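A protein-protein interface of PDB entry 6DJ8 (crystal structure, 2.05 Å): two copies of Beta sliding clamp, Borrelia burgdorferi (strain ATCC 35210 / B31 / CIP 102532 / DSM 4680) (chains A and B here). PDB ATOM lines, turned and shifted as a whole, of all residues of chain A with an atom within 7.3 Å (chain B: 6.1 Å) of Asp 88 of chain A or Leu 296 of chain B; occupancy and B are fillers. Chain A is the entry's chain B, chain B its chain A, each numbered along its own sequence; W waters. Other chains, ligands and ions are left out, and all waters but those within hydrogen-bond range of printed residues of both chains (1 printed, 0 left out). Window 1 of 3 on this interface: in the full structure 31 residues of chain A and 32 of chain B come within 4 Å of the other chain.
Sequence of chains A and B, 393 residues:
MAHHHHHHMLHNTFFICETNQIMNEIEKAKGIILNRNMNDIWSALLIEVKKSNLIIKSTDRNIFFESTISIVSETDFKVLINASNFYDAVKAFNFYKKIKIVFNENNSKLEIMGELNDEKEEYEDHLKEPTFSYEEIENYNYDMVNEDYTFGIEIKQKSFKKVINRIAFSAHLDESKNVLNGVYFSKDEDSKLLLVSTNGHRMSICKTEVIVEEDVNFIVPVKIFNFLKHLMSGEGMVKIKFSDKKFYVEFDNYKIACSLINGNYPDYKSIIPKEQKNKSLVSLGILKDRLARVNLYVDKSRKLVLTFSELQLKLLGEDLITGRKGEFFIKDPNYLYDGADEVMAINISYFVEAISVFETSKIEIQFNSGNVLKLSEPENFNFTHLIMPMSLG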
ATOM      1  N   ILE A  26      11.592  27.794  27.225  1.00  0.00           N
ATOM      2  CA  ILE A  26      11.070  26.735  28.089  1.00  0.00           C
ATOM      3  C   ILE A  26      11.462  26.986  29.543  1.00  0.00           C
ATOM      4  O   ILE A  26      10.652  26.805  30.461  1.00  0.00           O
ATOM      5  CB  ILE A  26      11.579  25.357  27.625  1.00  0.00           C
ATOM      6  CG1 ILE A  26      10.932  24.928  26.314  1.00  0.00           C
ATOM      7  CG2 ILE A  26      11.344  24.320  28.710  1.00  0.00           C
ATOM      8  CD1 ILE A  26      11.740  23.818  25.622  1.00  0.00           C
ATOM      9  N   LYS A  30       8.500  27.372  32.403  1.00  0.00           N
ATOM     10  CA  LYS A  30       8.269  26.402  33.462  1.00  0.00           C
ATOM     11  C   LYS A  30       8.506  26.980  34.847  1.00  0.00           C
ATOM     12  O   LYS A  30       8.280  26.277  35.834  1.00  0.00           O
ATOM     13  CB  LYS A  30       9.119  25.138  33.240  1.00  0.00           C
ATOM     14  CG  LYS A  30      10.512  25.176  33.778  1.00  0.00           C
ATOM     15  CD  LYS A  30      11.321  23.954  33.293  1.00  0.00           C
ATOM     16  CE  LYS A  30      12.095  23.337  34.443  1.00  0.00           C
ATOM     17  NZ  LYS A  30      12.947  24.321  35.162  1.00  0.00           N
ATOM     18  N   ASN A  82       5.475  17.001  29.787  1.00  0.00           N
ATOM     19  CA  ASN A  82       6.088  17.332  31.077  1.00  0.00           C
ATOM     20  C   ASN A  82       7.176  18.380  30.884  1.00  0.00           C
ATOM     21  O   ASN A  82       8.072  18.219  30.050  1.00  0.00           O
ATOM     22  CB  ASN A  82       6.674  16.064  31.722  1.00  0.00           C
ATOM     23  CG  ASN A  82       7.402  16.366  33.030  1.00  0.00           C
ATOM     24  OD1 ASN A  82       8.624  16.511  33.047  1.00  0.00           O
ATOM     25  ND2 ASN A  82       6.652  16.467  34.127  1.00  0.00           N
ATOM     26  N   ALA A  83       7.065  19.487  31.628  1.00  0.00           N
ATOM     27  CA  ALA A  83       7.922  20.639  31.356  1.00  0.00           C
ATOM     28  C   ALA A  83       9.375  20.352  31.701  1.00  0.00           C
ATOM     29  O   ALA A  83      10.282  20.747  30.962  1.00  0.00           O
ATOM     30  CB  ALA A  83       7.431  21.875  32.122  1.00  0.00           C
ATOM     31  N   SER A  84       9.616  19.692  32.832  1.00  0.00           N
ATOM     32  CA  SER A  84      10.989  19.425  33.253  1.00  0.00           C
ATOM     33  C   SER A  84      11.707  18.498  32.267  1.00  0.00           C
ATOM     34  O   SER A  84      12.878  18.725  31.933  1.00  0.00           O
ATOM     35  CB  SER A  84      10.982  18.833  34.666  1.00  0.00           C
ATOM     36  OG  SER A  84      12.294  18.502  35.076  1.00  0.00           O
ATOM     37  N   ASN A  85      11.026  17.448  31.796  1.00  0.00           N
ATOM     38  CA  ASN A  85      11.641  16.546  30.826  1.00  0.00           C
ATOM     39  C   ASN A  85      11.926  17.263  29.506  1.00  0.00           C
ATOM     40  O   ASN A  85      12.988  17.077  28.903  1.00  0.00           O
ATOM     41  CB  ASN A  85      10.743  15.329  30.580  1.00  0.00           C
ATOM     42  CG  ASN A  85      10.669  14.396  31.769  1.00  0.00           C
ATOM     43  OD1 ASN A  85      11.440  14.504  32.720  1.00  0.00           O
ATOM     44  ND2 ASN A  85       9.724  13.481  31.726  1.00  0.00           N
ATOM     45  N   PHE A  86      10.992  18.088  29.042  1.00  0.00           N
ATOM     46  CA  PHE A  86      11.219  18.821  27.801  1.00  0.00           C
ATOM     47  C   PHE A  86      12.411  19.763  27.935  1.00  0.00           C
ATOM     48  O   PHE A  86      13.247  19.859  27.029  1.00  0.00           O
ATOM     49  CB  PHE A  86       9.961  19.605  27.421  1.00  0.00           C
ATOM     50  CG  PHE A  86       9.974  20.140  26.014  1.00  0.00           C
ATOM     51  CD1 PHE A  86      10.638  19.464  25.002  1.00  0.00           C
ATOM     52  CD2 PHE A  86       9.295  21.317  25.696  1.00  0.00           C
ATOM     53  CE1 PHE A  86      10.645  19.946  23.705  1.00  0.00           C
ATOM     54  CE2 PHE A  86       9.277  21.792  24.387  1.00  0.00           C
ATOM     55  CZ  PHE A  86       9.961  21.117  23.394  1.00  0.00           C
ATOM     56  N   TYR A  87      12.499  20.472  29.060  1.00  0.00           N
ATOM     57  CA  TYR A  87      13.657  21.322  29.299  1.00  0.00           C
ATOM     58  C   TYR A  87      14.946  20.509  29.286  1.00  0.00           C
ATOM     59  O   TYR A  87      15.939  20.918  28.679  1.00  0.00           O
ATOM     60  CB  TYR A  87      13.519  22.059  30.629  1.00  0.00           C
ATOM     61  CG  TYR A  87      14.687  22.971  30.905  1.00  0.00           C
ATOM     62  CD1 TYR A  87      15.038  23.960  30.006  1.00  0.00           C
ATOM     63  CD2 TYR A  87      15.412  22.869  32.081  1.00  0.00           C
ATOM     64  CE1 TYR A  87      16.092  24.810  30.259  1.00  0.00           C
ATOM     65  CE2 TYR A  87      16.473  23.722  32.345  1.00  0.00           C
ATOM     66  CZ  TYR A  87      16.805  24.687  31.426  1.00  0.00           C
ATOM     67  OH  TYR A  87      17.857  25.542  31.659  1.00  0.00           O
ATOM     68  N   ASP A  88      14.952  19.364  29.966  1.00  0.00           N
ATOM     69  CA  ASP A  88      16.157  18.528  29.988  1.00  0.00           C
ATOM     70  C   ASP A  88      16.556  18.085  28.577  1.00  0.00           C
ATOM     71  O   ASP A  88      17.740  18.089  28.224  1.00  0.00           O
ATOM     72  CB  ASP A  88      15.932  17.316  30.884  1.00  0.00           C
ATOM     73  CG  ASP A  88      15.972  17.664  32.346  1.00  0.00           C
ATOM     74  OD1 ASP A  88      16.327  18.818  32.675  1.00  0.00           O
ATOM     75  OD2 ASP A  88      15.676  16.775  33.163  1.00  0.00           O
ATOM     76  N   ALA A  89      15.576  17.707  27.757  1.00  0.00           N
ATOM     77  CA  ALA A  89      15.855  17.286  26.388  1.00  0.00           C
ATOM     78  C   ALA A  89      16.570  18.382  25.607  1.00  0.00           C
ATOM     79  O   ALA A  89      17.623  18.156  24.997  1.00  0.00           O
ATOM     80  CB  ALA A  89      14.545  16.899  25.695  1.00  0.00           C
ATOM     81  N   VAL A  90      16.027  19.594  25.645  1.00  0.00           N
ATOM     82  CA  VAL A  90      16.617  20.682  24.878  1.00  0.00           C
ATOM     83  C   VAL A  90      17.984  21.062  25.440  1.00  0.00           C
ATOM     84  O   VAL A  90      18.919  21.351  24.686  1.00  0.00           O
ATOM     85  CB  VAL A  90      15.632  21.864  24.841  1.00  0.00           C
ATOM     86  CG1 VAL A  90      16.331  23.121  24.416  1.00  0.00           C
ATOM     87  CG2 VAL A  90      14.492  21.525  23.864  1.00  0.00           C
ATOM     88  N   LYS A  91      18.136  21.035  26.766  1.00  0.00           N
ATOM     89  CA  LYS A  91      19.463  21.200  27.372  1.00  0.00           C
ATOM     90  C   LYS A  91      20.429  20.113  26.917  1.00  0.00           C
ATOM     91  O   LYS A  91      21.615  20.372  26.670  1.00  0.00           O
ATOM     92  CB  LYS A  91      19.359  21.135  28.900  1.00  0.00           C
ATOM     93  CG  LYS A  91      19.300  22.434  29.681  1.00  0.00           C
ATOM     94  CD  LYS A  91      19.284  22.100  31.194  1.00  0.00           C
ATOM     95  CE  LYS A  91      20.643  21.576  31.676  1.00  0.00           C
ATOM     96  NZ  LYS A  91      21.430  22.491  32.562  1.00  0.00           N
ATOM     97  N   ALA A  92      19.955  18.873  26.857  1.00  0.00           N
ATOM     98  CA  ALA A  92      20.824  17.776  26.446  1.00  0.00           C
ATOM     99  C   ALA A  92      21.404  18.023  25.059  1.00  0.00           C
ATOM    100  O   ALA A  92      22.542  17.630  24.783  1.00  0.00           O
ATOM    101  CB  ALA A  92      20.046  16.460  26.492  1.00  0.00           C
ATOM    102  N   PHE A  93      20.655  18.698  24.181  1.00  0.00           N
ATOM    103  CA  PHE A  93      21.093  18.943  22.813  1.00  0.00           C
ATOM    104  C   PHE A  93      21.618  20.359  22.592  1.00  0.00           C
ATOM    105  O   PHE A  93      21.623  20.834  21.450  1.00  0.00           O
ATOM    106  CB  PHE A  93      19.956  18.644  21.832  1.00  0.00           C
ATOM    107  CG  PHE A  93      19.948  17.233  21.336  1.00  0.00           C
ATOM    108  CD1 PHE A  93      20.743  16.265  21.942  1.00  0.00           C
ATOM    109  CD2 PHE A  93      19.198  16.879  20.236  1.00  0.00           C
ATOM    110  CE1 PHE A  93      20.747  14.971  21.475  1.00  0.00           C
ATOM    111  CE2 PHE A  93      19.200  15.586  19.768  1.00  0.00           C
ATOM    112  CZ  PHE A  93      19.979  14.632  20.384  1.00  0.00           C
ATOM    113  N   ASN A  94      22.058  21.044  23.654  1.00  0.00           N
ATOM    114  CA  ASN A  94      22.531  22.414  23.499  1.00  0.00           C
ATOM    115  C   ASN A  94      23.768  22.520  22.620  1.00  0.00           C
ATOM    116  O   ASN A  94      24.162  23.634  22.262  1.00  0.00           O
ATOM    117  CB  ASN A  94      22.781  23.041  24.876  1.00  0.00           C
ATOM    118  CG  ASN A  94      23.883  22.371  25.643  1.00  0.00           C
ATOM    119  OD1 ASN A  94      24.969  22.137  25.125  1.00  0.00           O
ATOM    120  ND2 ASN A  94      23.605  22.041  26.901  1.00  0.00           N
ATOM    121  N   ILE A 112      13.657  14.149  19.235  1.00  0.00           N
ATOM    122  CA  ILE A 112      14.528  15.280  18.954  1.00  0.00           C
ATOM    123  C   ILE A 112      15.813  14.783  18.306  1.00  0.00           C
ATOM    124  O   ILE A 112      16.380  13.763  18.719  1.00  0.00           O
ATOM    125  CB  ILE A 112      14.816  16.084  20.237  1.00  0.00           C
ATOM    126  CG1 ILE A 112      13.499  16.387  20.953  1.00  0.00           C
ATOM    127  CG2 ILE A 112      15.531  17.382  19.910  1.00  0.00           C
ATOM    128  CD1 ILE A 112      13.644  17.347  22.115  1.00  0.00           C
ATOM    129  N   LEU A 127      16.783  11.691  20.883  1.00  0.00           N
ATOM    130  CA  LEU A 127      16.051  11.700  22.144  1.00  0.00           C
ATOM    131  C   LEU A 127      14.592  11.339  21.905  1.00  0.00           C
ATOM    132  O   LEU A 127      14.012  11.708  20.882  1.00  0.00           O
ATOM    133  CB  LEU A 127      16.103  13.074  22.837  1.00  0.00           C
ATOM    134  CG  LEU A 127      17.429  13.835  22.875  1.00  0.00           C
ATOM    135  CD1 LEU A 127      17.211  15.196  23.531  1.00  0.00           C
ATOM    136  CD2 LEU A 127      18.544  13.015  23.591  1.00  0.00           C
ATOM    137  N   GLU A 129      10.984  11.559  24.067  1.00  0.00           N
ATOM    138  CA  GLU A 129      10.287  12.129  25.225  1.00  0.00           C
ATOM    139  C   GLU A 129       8.817  11.738  25.202  1.00  0.00           C
ATOM    140  O   GLU A 129       8.111  12.063  24.231  1.00  0.00           O
ATOM    141  CB  GLU A 129      10.413  13.655  25.241  1.00  0.00           C
ATOM    142  CG  GLU A 129      11.811  14.166  25.532  1.00  0.00           C
ATOM    143  CD  GLU A 129      12.221  13.966  26.969  1.00  0.00           C
ATOM    144  OE1 GLU A 129      11.356  13.615  27.799  1.00  0.00           O
ATOM    145  OE2 GLU A 129      13.422  14.132  27.276  1.00  0.00           O
ATOM    146  N   LEU B 291      28.611  12.390  28.668  1.00  0.00           N
ATOM    147  CA  LEU B 291      28.085  11.736  29.862  1.00  0.00           C
ATOM    148  C   LEU B 291      27.175  12.679  30.631  1.00  0.00           C
ATOM    149  O   LEU B 291      26.181  12.250  31.232  1.00  0.00           O
ATOM    150  CB  LEU B 291      29.231  11.246  30.768  1.00  0.00           C
ATOM    151  CG  LEU B 291      29.958  10.023  30.199  1.00  0.00           C
ATOM    152  CD1 LEU B 291      31.200   9.696  31.022  1.00  0.00           C
ATOM    153  CD2 LEU B 291      29.014   8.835  30.175  1.00  0.00           C
ATOM    154  N   ALA B 292      27.520  13.966  30.650  1.00  0.00           N
ATOM    155  CA  ALA B 292      26.657  14.927  31.328  1.00  0.00           C
ATOM    156  C   ALA B 292      25.318  15.060  30.613  1.00  0.00           C
ATOM    157  O   ALA B 292      24.293  15.322  31.253  1.00  0.00           O
ATOM    158  CB  ALA B 292      27.354  16.283  31.441  1.00  0.00           C
ATOM    159  N   ARG B 293      25.302  14.879  29.292  1.00  0.00           N
ATOM    160  CA  ARG B 293      24.039  14.976  28.572  1.00  0.00           C
ATOM    161  C   ARG B 293      23.220  13.699  28.721  1.00  0.00           C
ATOM    162  O   ARG B 293      22.022  13.763  29.022  1.00  0.00           O
ATOM    163  CB  ARG B 293      24.298  15.305  27.110  1.00  0.00           C
ATOM    164  CG  ARG B 293      25.035  16.607  26.964  1.00  0.00           C
ATOM    165  CD  ARG B 293      25.550  16.810  25.561  1.00  0.00           C
ATOM    166  NE  ARG B 293      26.450  17.950  25.534  1.00  0.00           N
ATOM    167  CZ  ARG B 293      26.022  19.207  25.543  1.00  0.00           C
ATOM    168  NH1 ARG B 293      26.891  20.203  25.526  1.00  0.00           N
ATOM    169  NH2 ARG B 293      24.715  19.457  25.580  1.00  0.00           N
ATOM    170  N   VAL B 294      23.851  12.528  28.538  1.00  0.00           N
ATOM    171  CA  VAL B 294      23.094  11.280  28.629  1.00  0.00           C
ATOM    172  C   VAL B 294      22.640  11.050  30.059  1.00  0.00           C
ATOM    173  O   VAL B 294      21.587  10.437  30.297  1.00  0.00           O
ATOM    174  CB  VAL B 294      23.924  10.086  28.084  1.00  0.00           C
ATOM    175  CG1 VAL B 294      24.977   9.607  29.101  1.00  0.00           C
ATOM    176  CG2 VAL B 294      23.019   8.930  27.727  1.00  0.00           C
ATOM    177  N   ASN B 295      23.379  11.591  31.032  1.00  0.00           N
ATOM    178  CA  ASN B 295      22.948  11.535  32.425  1.00  0.00           C
ATOM    179  C   ASN B 295      21.514  12.028  32.595  1.00  0.00           C
ATOM    180  O   ASN B 295      20.812  11.578  33.504  1.00  0.00           O
ATOM    181  CB  ASN B 295      23.858  12.395  33.301  1.00  0.00           C
ATOM    182  CG  ASN B 295      23.543  12.253  34.773  1.00  0.00           C
ATOM    183  OD1 ASN B 295      23.476  11.142  35.297  1.00  0.00           O
ATOM    184  ND2 ASN B 295      23.300  13.387  35.442  1.00  0.00           N
ATOM    185  N   LEU B 296      21.053  12.935  31.727  1.00  0.00           N
ATOM    186  CA  LEU B 296      19.688  13.440  31.881  1.00  0.00           C
ATOM    187  C   LEU B 296      18.649  12.387  31.539  1.00  0.00           C
ATOM    188  O   LEU B 296      17.452  12.634  31.735  1.00  0.00           O
ATOM    189  CB  LEU B 296      19.494  14.685  31.012  1.00  0.00           C
ATOM    190  CG  LEU B 296      20.332  15.876  31.489  1.00  0.00           C
ATOM    191  CD1 LEU B 296      20.353  16.982  30.443  1.00  0.00           C
ATOM    192  CD2 LEU B 296      19.785  16.405  32.813  1.00  0.00           C
ATOM    193  N   TYR B 297      19.089  11.219  31.055  1.00  0.00           N
ATOM    194  CA  TYR B 297      18.215  10.120  30.671  1.00  0.00           C
ATOM    195  C   TYR B 297      18.501   8.841  31.445  1.00  0.00           C
ATOM    196  O   TYR B 297      18.045   7.760  31.043  1.00  0.00           O
ATOM    197  CB  TYR B 297      18.328   9.861  29.164  1.00  0.00           C
ATOM    198  CG  TYR B 297      17.703  10.988  28.388  1.00  0.00           C
ATOM    199  CD1 TYR B 297      18.442  12.111  28.043  1.00  0.00           C
ATOM    200  CD2 TYR B 297      16.348  10.957  28.058  1.00  0.00           C
ATOM    201  CE1 TYR B 297      17.849  13.175  27.360  1.00  0.00           C
ATOM    202  CE2 TYR B 297      15.745  12.019  27.387  1.00  0.00           C
ATOM    203  CZ  TYR B 297      16.497  13.117  27.040  1.00  0.00           C
ATOM    204  OH  TYR B 297      15.898  14.156  26.358  1.00  0.00           O
ATOM    205  N   VAL B 298      19.267   8.922  32.518  1.00  0.00           N
ATOM    206  CA  VAL B 298      19.575   7.775  33.358  1.00  0.00           C
ATOM    207  C   VAL B 298      18.792   7.914  34.656  1.00  0.00           C
ATOM    208  O   VAL B 298      18.709   9.008  35.218  1.00  0.00           O
ATOM    209  CB  VAL B 298      21.089   7.671  33.625  1.00  0.00           C
ATOM    210  CG1 VAL B 298      21.362   6.517  34.571  1.00  0.00           C
ATOM    211  CG2 VAL B 298      21.843   7.470  32.294  1.00  0.00           C
ATOM    212  N   ARG B 324      11.050   6.902  27.824  1.00  0.00           N
ATOM    213  CA  ARG B 324      11.969   8.024  27.708  1.00  0.00           C
ATOM    214  C   ARG B 324      13.396   7.529  27.497  1.00  0.00           C
ATOM    215  O   ARG B 324      13.882   6.667  28.237  1.00  0.00           O
ATOM    216  CB  ARG B 324      11.910   8.884  28.966  1.00  0.00           C
ATOM    217  CG  ARG B 324      12.622  10.193  28.809  1.00  0.00           C
ATOM    218  CD  ARG B 324      12.220  11.195  29.897  1.00  0.00           C
ATOM    219  NE  ARG B 324      12.886  12.458  29.632  1.00  0.00           N
ATOM    220  CZ  ARG B 324      14.041  12.818  30.183  1.00  0.00           C
ATOM    221  NH1 ARG B 324      14.584  13.986  29.867  1.00  0.00           N
ATOM    222  NH2 ARG B 324      14.641  12.020  31.058  1.00  0.00           N
HETATM  223  O   HOH W   1      16.462  14.272  33.626  1.00  0.00           O
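Hydrophobic or aromatic side chains of chain B within 4 Å of the printed part of chain A: Leu 296 and Tyr 297.
Along chain B the printed residues that touch a printed residue of chain A span positions 293 to 324.
Hydrophobic or aromatic side chains of chain A that line the printed part of chain B: Ala 89, Ala 92 and Leu 127.
Among the printed residues, Asp or Glu carboxylates within 4 Å of a Lys or Arg side-chain nitrogen of the other chain: Glu 129 of chain A with Arg 324 of chain B.
Among the printed residues, merely in contact across the chains: Asn 85 of chain A with Arg 324 of chain B, Asp 88 of chain A with Leu 296 of chain B, Asp 88 of chain A with Arg 324 of chain B, Ala 89 of chain A with Tyr 297 of chain B, Ala 92 of chain A with Leu 296 of chain B and Leu 127 of chain A with Tyr 297 of chain B.
No position is printed for both chains.
Of the 11 pairs that touch across the chains among the printed residues, none has its exchanged pair printed and touching as well.
O of Lys 91 of chain A is in hydrogen-bond range of NH2 of Arg 293 of chain B (3.4 Å).
NH2 of Arg 293 of chain B sits at hydrogen-bond distance from O of Ala 92 of chain A (2.9 Å).
NH2 of Arg 293 of chain B sits at hydrogen-bond distance from OD1 of Asn 94 of chain A (2.7 Å).
The side-chain hydroxyl (OH) of Tyr 297 of chain B is in hydrogen-bond range of the side-chain carboxylate (OE2) of Glu 129 of chain A, 2.6 Å away.
The guanidinium group (NE) of Arg 324 of chain B is in salt-bridge range of the side-chain carboxylate (OE1) of Glu 129 of chain A (2.7 Å).
Water W1 bridges OD2 of Asp 88 of chain A (2.7 Å) and O of Leu 296 of chain B (2.7 Å).
Printed residues of chain B within 4 Å of Asn 85 of chain A: Arg 324 (3.6 Å).
Of the printed residues of chain B, Asp 88 of chain A touches Leu 296 and Arg 324.
Of the printed residues of chain B, Ala 89 of chain A touches Tyr 297.
Printed residues of chain B within 4 Å of Ala 92 of chain A: Arg 293 and Leu 296.
Phe 93 of chain A touches none of the printed residues of chain B.
Printed residues of chain B within 4 Å of Glu 129 of chain A: Tyr 297 (2.6 Å) and Arg 324 (2.7 Å).
Printed residues of chain A within 4 Å of Leu 296 of chain B: Asp 88 (3.6 Å) and Ala 92 (3.997 Å).
Val 298 of chain B touches none of the printed residues of chain A.
The nearest printed residue of chain A that does not touch Leu 296 of chain B is Lys 91 of chain A (4.5 Å).
The nearest printed residue of chain A that does not touch Arg 293 of chain B is Phe 93 of chain A (4.4 Å).
The backbone carbonyl oxygen (O) of Leu 296 of chain B sits at hydrogen-bond distance from the guanidinium group (NH2) of Arg 324 of chain B (3.0 Å).
N of Asn 85 of chain A sits at hydrogen-bond distance from OD1 of Asn 82 of chain A (2.9 Å).
O of Lys 91 of chain A sits at hydrogen-bond distance from ND2 of Asn 94 of chain A, at 2.6 Å.
N of Ile 112 of chain A lies within hydrogen-bond range of O of Leu 127 of chain A (3.0 Å).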
